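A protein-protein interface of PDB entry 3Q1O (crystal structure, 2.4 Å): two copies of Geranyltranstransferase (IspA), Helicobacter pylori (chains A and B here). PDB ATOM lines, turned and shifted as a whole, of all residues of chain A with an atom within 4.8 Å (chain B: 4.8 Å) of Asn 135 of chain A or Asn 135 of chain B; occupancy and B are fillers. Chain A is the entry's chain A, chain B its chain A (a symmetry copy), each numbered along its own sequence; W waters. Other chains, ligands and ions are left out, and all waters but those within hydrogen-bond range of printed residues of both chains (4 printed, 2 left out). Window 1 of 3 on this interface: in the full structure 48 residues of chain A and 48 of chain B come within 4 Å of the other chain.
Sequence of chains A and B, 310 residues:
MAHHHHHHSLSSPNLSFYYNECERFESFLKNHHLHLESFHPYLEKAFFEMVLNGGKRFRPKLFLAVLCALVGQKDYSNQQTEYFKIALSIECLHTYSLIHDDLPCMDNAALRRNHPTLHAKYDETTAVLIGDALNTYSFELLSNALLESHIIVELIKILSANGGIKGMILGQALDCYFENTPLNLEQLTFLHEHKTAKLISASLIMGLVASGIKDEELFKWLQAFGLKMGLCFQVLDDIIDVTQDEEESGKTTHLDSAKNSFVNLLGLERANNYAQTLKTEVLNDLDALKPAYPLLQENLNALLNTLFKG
The backbone carbonyl oxygen (O) of Asp 132 of chain A sits close to the side-chain amide oxygen (OD1) of Asn 135 of chain B. OD1 of Asn 135 of chain A sits close to O of Asp 132 of chain B (3.3 Å). The side-chain amide oxygen (OD1) of Asn 135 of chain B sits close to the side-chain amide oxygen (OD1) of Asn 135 of chain A (3.3 Å). ND2 of Asn 135 of chain A sits at hydrogen-bond distance from OG1 of Thr 136 of chain B (2.8 Å). The side-chain hydroxyl (OG1) of Thr 136 of chain A is in hydrogen-bond range of the side-chain amide nitrogen (ND2) of Asn 135 of chain B. OD1 of Asp 132 of chain A sits close to OD1 of Asp 132 of chain B, at 3.2 Å.
The backbone carbonyl oxygen of Asp 132 of chain A sits at hydrogen-bond distance from the side-chain hydroxyl of Thr 136 of chain A. The backbone carbonyl oxygen (O) of Asn 135 of chain A lies close to the side-chain hydroxyl (OG) of Ser 138 of chain A (3.5 Å). OG1 of Thr 136 of chain B sits at hydrogen-bond distance from O of Asp 132 of chain B (3.1 Å). The backbone carbonyl oxygen (O) of Asn 135 of chain B lies close to the side-chain hydroxyl (OG) of Ser 138 of chain B (3.5 Å).
OH of Tyr 96 of chain A touches CB of Asp 132 of chain B (3.2 Å). OH of Tyr 96 of chain B touches CB of Asp 132 of chain A (3.2 Å). Thr 136 of chain A touches Phe 139 of chain B. CZ of Phe 139 of chain A touches CG2 of Thr 136 of chain B, at 3.8 Å. Phe 139 of chain A touches Phe 139 of chain B.
Of chain B, only Asp 132 (3.3 Å), Asn 135 (3.3 Å) and Thr 136 (2.8 Å) come within 4 Å of Asn 135 of chain A. Of the printed residues of chain B, Phe 139 of chain A touches Thr 136 and Phe 139. Ala 133 of chain B touches none of the printed residues of chain A. Asn 135 of chain B touches just these residues of chain A: Asp 132 (3.3 Å), Asn 135 (3.3 Å) and Thr 136 (2.8 Å). Of the printed residues of chain A, Thr 136 of chain B touches Asn 135 (2.8 Å) and Phe 139 (3.8 Å). The nearest printed residue of chain B that does not touch Asn 135 of chain A is Ala 133 of chain B (5.3 Å). The nearest printed residue of chain A that does not touch Asn 135 of chain B is Ala 133 of chain A (5.3 Å).
Hydrophobic or aromatic side chains of chain B within 4 Å of the printed part of chain A: Tyr 96 and Phe 139. Among the printed residues, 11 pairs touch across the chains. Among the printed residues, no Asp or Glu carboxylate lies within 4 Å of a Lys or Arg side-chain nitrogen of the other chain.
Tyr 96 of chain A touches Asp 132 of chain B, and with the chains exchanged Asp 132 of chain A touches Tyr 96 of chain B. Asp 132 of chain B touches its own counterpart, Asp 132 of chain A. Asn 135 of chain A touches Thr 136 of chain B, and with the chains exchanged Thr 136 of chain A touches Asn 135 of chain B. Phe 139 of chain B touches its own counterpart, Phe 139 of chain A. 11 positions are printed for both chains.
Water W3 bridges the side-chain hydroxyl of Tyr 96 of chain A and the side-chain hydroxyl of Thr 136 of chain B. Water W1 lies within hydrogen-bond range of OH of Tyr 96 of chain B and OG1 of Thr 136 of chain A. Water W2 lies within hydrogen-bond range of OD2 of Asp 132 of chain B (2.9 Å) and OH of Tyr 96 of chain A (3.1 Å). Water W4 bridges the side-chain carboxylate of Asp 132 of chain A (2.9 Å) and the side-chain hydroxyl of Tyr 96 of chain B (3.1 Å).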
ATOM      1  N   LEU A  93     -25.339  17.834   6.647  1.00  0.00           N
ATOM      2  CA  LEU A  93     -26.080  16.807   5.917  1.00  0.00           C
ATOM      3  C   LEU A  93     -27.509  17.247   5.633  1.00  0.00           C
ATOM      4  O   LEU A  93     -27.999  17.057   4.526  1.00  0.00           O
ATOM      5  CB  LEU A  93     -26.067  15.459   6.648  1.00  0.00           C
ATOM      6  CG  LEU A  93     -26.474  14.279   5.756  1.00  0.00           C
ATOM      7  CD1 LEU A  93     -25.255  13.581   5.203  1.00  0.00           C
ATOM      8  CD2 LEU A  93     -27.320  13.295   6.514  1.00  0.00           C
ATOM      9  N   TYR A  96     -27.265  19.942   2.883  1.00  0.00           N
ATOM     10  CA  TYR A  96     -27.041  19.261   1.604  1.00  0.00           C
ATOM     11  C   TYR A  96     -28.354  18.771   0.974  1.00  0.00           C
ATOM     12  O   TYR A  96     -28.568  18.960  -0.223  1.00  0.00           O
ATOM     13  CB  TYR A  96     -25.995  18.126   1.740  1.00  0.00           C
ATOM     14  CG  TYR A  96     -26.450  16.753   1.268  1.00  0.00           C
ATOM     15  CD1 TYR A  96     -26.687  16.483  -0.088  1.00  0.00           C
ATOM     16  CD2 TYR A  96     -26.643  15.716   2.183  1.00  0.00           C
ATOM     17  CE1 TYR A  96     -27.132  15.232  -0.509  1.00  0.00           C
ATOM     18  CE2 TYR A  96     -27.082  14.459   1.767  1.00  0.00           C
ATOM     19  CZ  TYR A  96     -27.321  14.228   0.420  1.00  0.00           C
ATOM     20  OH  TYR A  96     -27.746  12.994   0.001  1.00  0.00           O
ATOM     21  N   GLY A 131     -23.844  20.600  -2.711  1.00  0.00           N
ATOM     22  CA  GLY A 131     -24.642  19.576  -2.051  1.00  0.00           C
ATOM     23  C   GLY A 131     -23.807  18.340  -1.779  1.00  0.00           C
ATOM     24  O   GLY A 131     -23.741  17.862  -0.640  1.00  0.00           O
ATOM     25  N   ASP A 132     -23.132  17.857  -2.820  1.00  0.00           N
ATOM     26  CA  ASP A 132     -22.210  16.732  -2.712  1.00  0.00           C
ATOM     27  C   ASP A 132     -21.121  16.968  -1.677  1.00  0.00           C
ATOM     28  O   ASP A 132     -20.835  16.091  -0.858  1.00  0.00           O
ATOM     29  CB  ASP A 132     -21.578  16.451  -4.065  1.00  0.00           C
ATOM     30  CG  ASP A 132     -22.557  15.863  -5.047  1.00  0.00           C
ATOM     31  OD1 ASP A 132     -23.644  15.449  -4.602  1.00  0.00           O
ATOM     32  OD2 ASP A 132     -22.247  15.811  -6.258  1.00  0.00           O
ATOM     33  N   ALA A 133     -20.526  18.158  -1.722  1.00  0.00           N
ATOM     34  CA  ALA A 133     -19.480  18.552  -0.790  1.00  0.00           C
ATOM     35  C   ALA A 133     -19.959  18.543   0.661  1.00  0.00           C
ATOM     36  O   ALA A 133     -19.257  18.043   1.532  1.00  0.00           O
ATOM     37  CB  ALA A 133     -18.893  19.922  -1.179  1.00  0.00           C
ATOM     38  N   LEU A 134     -21.156  19.069   0.913  1.00  0.00           N
ATOM     39  CA  LEU A 134     -21.684  19.102   2.279  1.00  0.00           C
ATOM     40  C   LEU A 134     -22.069  17.720   2.796  1.00  0.00           C
ATOM     41  O   LEU A 134     -21.919  17.434   3.990  1.00  0.00           O
ATOM     42  CB  LEU A 134     -22.839  20.091   2.398  1.00  0.00           C
ATOM     43  CG  LEU A 134     -22.381  21.556   2.367  1.00  0.00           C
ATOM     44  CD1 LEU A 134     -23.495  22.459   1.902  1.00  0.00           C
ATOM     45  CD2 LEU A 134     -21.875  22.013   3.724  1.00  0.00           C
ATOM     46  N   ASN A 135     -22.544  16.870   1.890  1.00  0.00           N
ATOM     47  CA  ASN A 135     -22.801  15.451   2.167  1.00  0.00           C
ATOM     48  C   ASN A 135     -21.526  14.788   2.712  1.00  0.00           C
ATOM     49  O   ASN A 135     -21.529  14.213   3.802  1.00  0.00           O
ATOM     50  CB  ASN A 135     -23.295  14.793   0.873  1.00  0.00           C
ATOM     51  CG  ASN A 135     -23.783  13.345   1.044  1.00  0.00           C
ATOM     52  OD1 ASN A 135     -24.241  12.732   0.072  1.00  0.00           O
ATOM     53  ND2 ASN A 135     -23.683  12.800   2.242  1.00  0.00           N
ATOM     54  N   THR A 136     -20.438  14.910   1.959  1.00  0.00           N
ATOM     55  CA  THR A 136     -19.151  14.331   2.320  1.00  0.00           C
ATOM     56  C   THR A 136     -18.562  15.032   3.550  1.00  0.00           C
ATOM     57  O   THR A 136     -17.981  14.379   4.423  1.00  0.00           O
ATOM     58  CB  THR A 136     -18.177  14.403   1.113  1.00  0.00           C
ATOM     59  OG1 THR A 136     -18.813  13.829  -0.036  1.00  0.00           O
ATOM     60  CG2 THR A 136     -16.889  13.645   1.381  1.00  0.00           C
ATOM     61  N   TYR A 137     -18.746  16.351   3.628  1.00  0.00           N
ATOM     62  CA  TYR A 137     -18.195  17.166   4.702  1.00  0.00           C
ATOM     63  C   TYR A 137     -18.734  16.821   6.086  1.00  0.00           C
ATOM     64  O   TYR A 137     -18.010  16.940   7.076  1.00  0.00           O
ATOM     65  CB  TYR A 137     -18.399  18.653   4.421  1.00  0.00           C
ATOM     66  CG  TYR A 137     -17.574  19.554   5.311  1.00  0.00           C
ATOM     67  CD1 TYR A 137     -18.187  20.494   6.150  1.00  0.00           C
ATOM     68  CD2 TYR A 137     -16.175  19.459   5.327  1.00  0.00           C
ATOM     69  CE1 TYR A 137     -17.422  21.332   6.971  1.00  0.00           C
ATOM     70  CE2 TYR A 137     -15.404  20.284   6.152  1.00  0.00           C
ATOM     71  CZ  TYR A 137     -16.034  21.215   6.966  1.00  0.00           C
ATOM     72  OH  TYR A 137     -15.275  22.022   7.772  1.00  0.00           O
ATOM     73  N   SER A 138     -20.000  16.403   6.139  1.00  0.00           N
ATOM     74  CA  SER A 138     -20.631  15.879   7.351  1.00  0.00           C
ATOM     75  C   SER A 138     -19.777  14.816   8.000  1.00  0.00           C
ATOM     76  O   SER A 138     -19.577  14.818   9.206  1.00  0.00           O
ATOM     77  CB  SER A 138     -21.986  15.267   7.012  1.00  0.00           C
ATOM     78  OG  SER A 138     -22.770  16.227   6.340  1.00  0.00           O
ATOM     79  N   PHE A 139     -19.255  13.910   7.188  1.00  0.00           N
ATOM     80  CA  PHE A 139     -18.451  12.829   7.724  1.00  0.00           C
ATOM     81  C   PHE A 139     -17.023  13.251   8.050  1.00  0.00           C
ATOM     82  O   PHE A 139     -16.436  12.732   9.003  1.00  0.00           O
ATOM     83  CB  PHE A 139     -18.575  11.600   6.826  1.00  0.00           C
ATOM     84  CG  PHE A 139     -19.995  11.175   6.649  1.00  0.00           C
ATOM     85  CD1 PHE A 139     -20.677  10.562   7.694  1.00  0.00           C
ATOM     86  CD2 PHE A 139     -20.688  11.464   5.477  1.00  0.00           C
ATOM     87  CE1 PHE A 139     -22.013  10.199   7.553  1.00  0.00           C
ATOM     88  CE2 PHE A 139     -22.018  11.097   5.332  1.00  0.00           C
ATOM     89  CZ  PHE A 139     -22.679  10.468   6.375  1.00  0.00           C
ATOM     90  N   LEU B  93     -17.660   5.661  -3.534  1.00  0.00           N
ATOM     91  CA  LEU B  93     -17.423   7.097  -3.672  1.00  0.00           C
ATOM     92  C   LEU B  93     -16.976   7.456  -5.082  1.00  0.00           C
ATOM     93  O   LEU B  93     -17.455   8.431  -5.647  1.00  0.00           O
ATOM     94  CB  LEU B  93     -16.414   7.616  -2.640  1.00  0.00           C
ATOM     95  CG  LEU B  93     -16.433   9.142  -2.484  1.00  0.00           C
ATOM     96  CD1 LEU B  93     -17.293   9.549  -1.311  1.00  0.00           C
ATOM     97  CD2 LEU B  93     -15.043   9.684  -2.304  1.00  0.00           C
ATOM     98  N   TYR B  96     -20.107   7.102  -7.310  1.00  0.00           N
ATOM     99  CA  TYR B  96     -20.948   8.284  -7.095  1.00  0.00           C
ATOM    100  C   TYR B  96     -20.498   9.476  -7.955  1.00  0.00           C
ATOM    101  O   TYR B  96     -21.336  10.138  -8.569  1.00  0.00           O
ATOM    102  CB  TYR B  96     -21.044   8.647  -5.592  1.00  0.00           C
ATOM    103  CG  TYR B  96     -20.655  10.076  -5.235  1.00  0.00           C
ATOM    104  CD1 TYR B  96     -21.435  11.170  -5.633  1.00  0.00           C
ATOM    105  CD2 TYR B  96     -19.501  10.332  -4.492  1.00  0.00           C
ATOM    106  CE1 TYR B  96     -21.058  12.475  -5.328  1.00  0.00           C
ATOM    107  CE2 TYR B  96     -19.120  11.638  -4.178  1.00  0.00           C
ATOM    108  CZ  TYR B  96     -19.906  12.700  -4.599  1.00  0.00           C
ATOM    109  OH  TYR B  96     -19.545  13.984  -4.289  1.00  0.00           O
ATOM    110  N   GLY B 131     -26.447   8.813  -6.749  1.00  0.00           N
ATOM    111  CA  GLY B 131     -25.143   9.426  -6.537  1.00  0.00           C
ATOM    112  C   GLY B 131     -24.982   9.854  -5.091  1.00  0.00           C
ATOM    113  O   GLY B 131     -24.003   9.485  -4.430  1.00  0.00           O
ATOM    114  N   ASP B 132     -25.971  10.592  -4.593  1.00  0.00           N
ATOM    115  CA  ASP B 132     -26.021  11.008  -3.195  1.00  0.00           C
ATOM    116  C   ASP B 132     -25.952   9.833  -2.233  1.00  0.00           C
ATOM    117  O   ASP B 132     -25.197   9.866  -1.258  1.00  0.00           O
ATOM    118  CB  ASP B 132     -27.289  11.806  -2.940  1.00  0.00           C
ATOM    119  CG  ASP B 132     -27.258  13.163  -3.592  1.00  0.00           C
ATOM    120  OD1 ASP B 132     -26.162  13.572  -4.025  1.00  0.00           O
ATOM    121  OD2 ASP B 132     -28.317  13.823  -3.674  1.00  0.00           O
ATOM    122  N   ALA B 133     -26.740   8.801  -2.522  1.00  0.00           N
ATOM    123  CA  ALA B 133     -26.779   7.588  -1.717  1.00  0.00           C
ATOM    124  C   ALA B 133     -25.423   6.885  -1.656  1.00  0.00           C
ATOM    125  O   ALA B 133     -24.998   6.472  -0.583  1.00  0.00           O
ATOM    126  CB  ALA B 133     -27.882   6.637  -2.217  1.00  0.00           C
ATOM    127  N   LEU B 134     -24.739   6.777  -2.793  1.00  0.00           N
ATOM    128  CA  LEU B 134     -23.434   6.112  -2.818  1.00  0.00           C
ATOM    129  C   LEU B 134     -22.346   6.924  -2.123  1.00  0.00           C
ATOM    130  O   LEU B 134     -21.442   6.355  -1.500  1.00  0.00           O
ATOM    131  CB  LEU B 134     -23.036   5.737  -4.242  1.00  0.00           C
ATOM    132  CG  LEU B 134     -23.832   4.548  -4.796  1.00  0.00           C
ATOM    133  CD1 LEU B 134     -23.861   4.572  -6.302  1.00  0.00           C
ATOM    134  CD2 LEU B 134     -23.269   3.223  -4.309  1.00  0.00           C
ATOM    135  N   ASN B 135     -22.453   8.247  -2.221  1.00  0.00           N
ATOM    136  CA  ASN B 135     -21.603   9.184  -1.476  1.00  0.00           C
ATOM    137  C   ASN B 135     -21.689   8.883   0.029  1.00  0.00           C
ATOM    138  O   ASN B 135     -20.675   8.637   0.683  1.00  0.00           O
ATOM    139  CB  ASN B 135     -22.055  10.610  -1.814  1.00  0.00           C
ATOM    140  CG  ASN B 135     -21.143  11.715  -1.254  1.00  0.00           C
ATOM    141  OD1 ASN B 135     -21.393  12.901  -1.501  1.00  0.00           O
ATOM    142  ND2 ASN B 135     -20.117  11.346  -0.510  1.00  0.00           N
ATOM    143  N   THR B 136     -22.912   8.869   0.551  1.00  0.00           N
ATOM    144  CA  THR B 136     -23.170   8.615   1.962  1.00  0.00           C
ATOM    145  C   THR B 136     -22.835   7.164   2.326  1.00  0.00           C
ATOM    146  O   THR B 136     -22.287   6.901   3.401  1.00  0.00           O
ATOM    147  CB  THR B 136     -24.648   8.952   2.300  1.00  0.00           C
ATOM    148  OG1 THR B 136     -24.940  10.280   1.848  1.00  0.00           O
ATOM    149  CG2 THR B 136     -24.915   8.881   3.794  1.00  0.00           C
ATOM    150  N   TYR B 137     -23.135   6.238   1.414  1.00  0.00           N
ATOM    151  CA  TYR B 137     -22.934   4.812   1.637  1.00  0.00           C
ATOM    152  C   TYR B 137     -21.477   4.411   1.837  1.00  0.00           C
ATOM    153  O   TYR B 137     -21.192   3.476   2.585  1.00  0.00           O
ATOM    154  CB  TYR B 137     -23.548   3.989   0.506  1.00  0.00           C
ATOM    155  CG  TYR B 137     -23.670   2.518   0.829  1.00  0.00           C
ATOM    156  CD1 TYR B 137     -23.027   1.552   0.044  1.00  0.00           C
ATOM    157  CD2 TYR B 137     -24.420   2.086   1.933  1.00  0.00           C
ATOM    158  CE1 TYR B 137     -23.144   0.189   0.339  1.00  0.00           C
ATOM    159  CE2 TYR B 137     -24.533   0.727   2.243  1.00  0.00           C
ATOM    160  CZ  TYR B 137     -23.895  -0.210   1.442  1.00  0.00           C
ATOM    161  OH  TYR B 137     -24.009  -1.541   1.749  1.00  0.00           O
ATOM    162  N   SER B 138     -20.571   5.123   1.162  1.00  0.00           N
ATOM    163  CA  SER B 138     -19.127   4.986   1.353  1.00  0.00           C
ATOM    164  C   SER B 138     -18.756   5.056   2.815  1.00  0.00           C
ATOM    165  O   SER B 138     -17.973   4.255   3.305  1.00  0.00           O
ATOM    166  CB  SER B 138     -18.394   6.104   0.617  1.00  0.00           C
ATOM    167  OG  SER B 138     -18.786   6.097  -0.737  1.00  0.00           O
ATOM    168  N   PHE B 139     -19.340   6.012   3.521  1.00  0.00           N
ATOM    169  CA  PHE B 139     -19.019   6.180   4.925  1.00  0.00           C
ATOM    170  C   PHE B 139     -19.735   5.181   5.826  1.00  0.00           C
ATOM    171  O   PHE B 139     -19.178   4.771   6.846  1.00  0.00           O
ATOM    172  CB  PHE B 139     -19.186   7.646   5.319  1.00  0.00           C
ATOM    173  CG  PHE B 139     -18.363   8.554   4.469  1.00  0.00           C
ATOM    174  CD1 PHE B 139     -16.982   8.601   4.629  1.00  0.00           C
ATOM    175  CD2 PHE B 139     -18.943   9.298   3.445  1.00  0.00           C
ATOM    176  CE1 PHE B 139     -16.201   9.414   3.813  1.00  0.00           C
ATOM    177  CE2 PHE B 139     -18.166  10.114   2.636  1.00  0.00           C
ATOM    178  CZ  PHE B 139     -16.793  10.165   2.820  1.00  0.00           C
HETATM  179  O   HOH W   1     -17.649  13.914  -2.458  1.00  0.00           O
HETATM  180  O   HOH W   2     -30.177  14.150  -1.466  1.00  0.00           O
HETATM  181  O   HOH W   3     -27.436  11.275   1.975  1.00  0.00           O
HETATM  182  O   HOH W   4     -19.661  14.896  -7.213  1.00  0.00           O
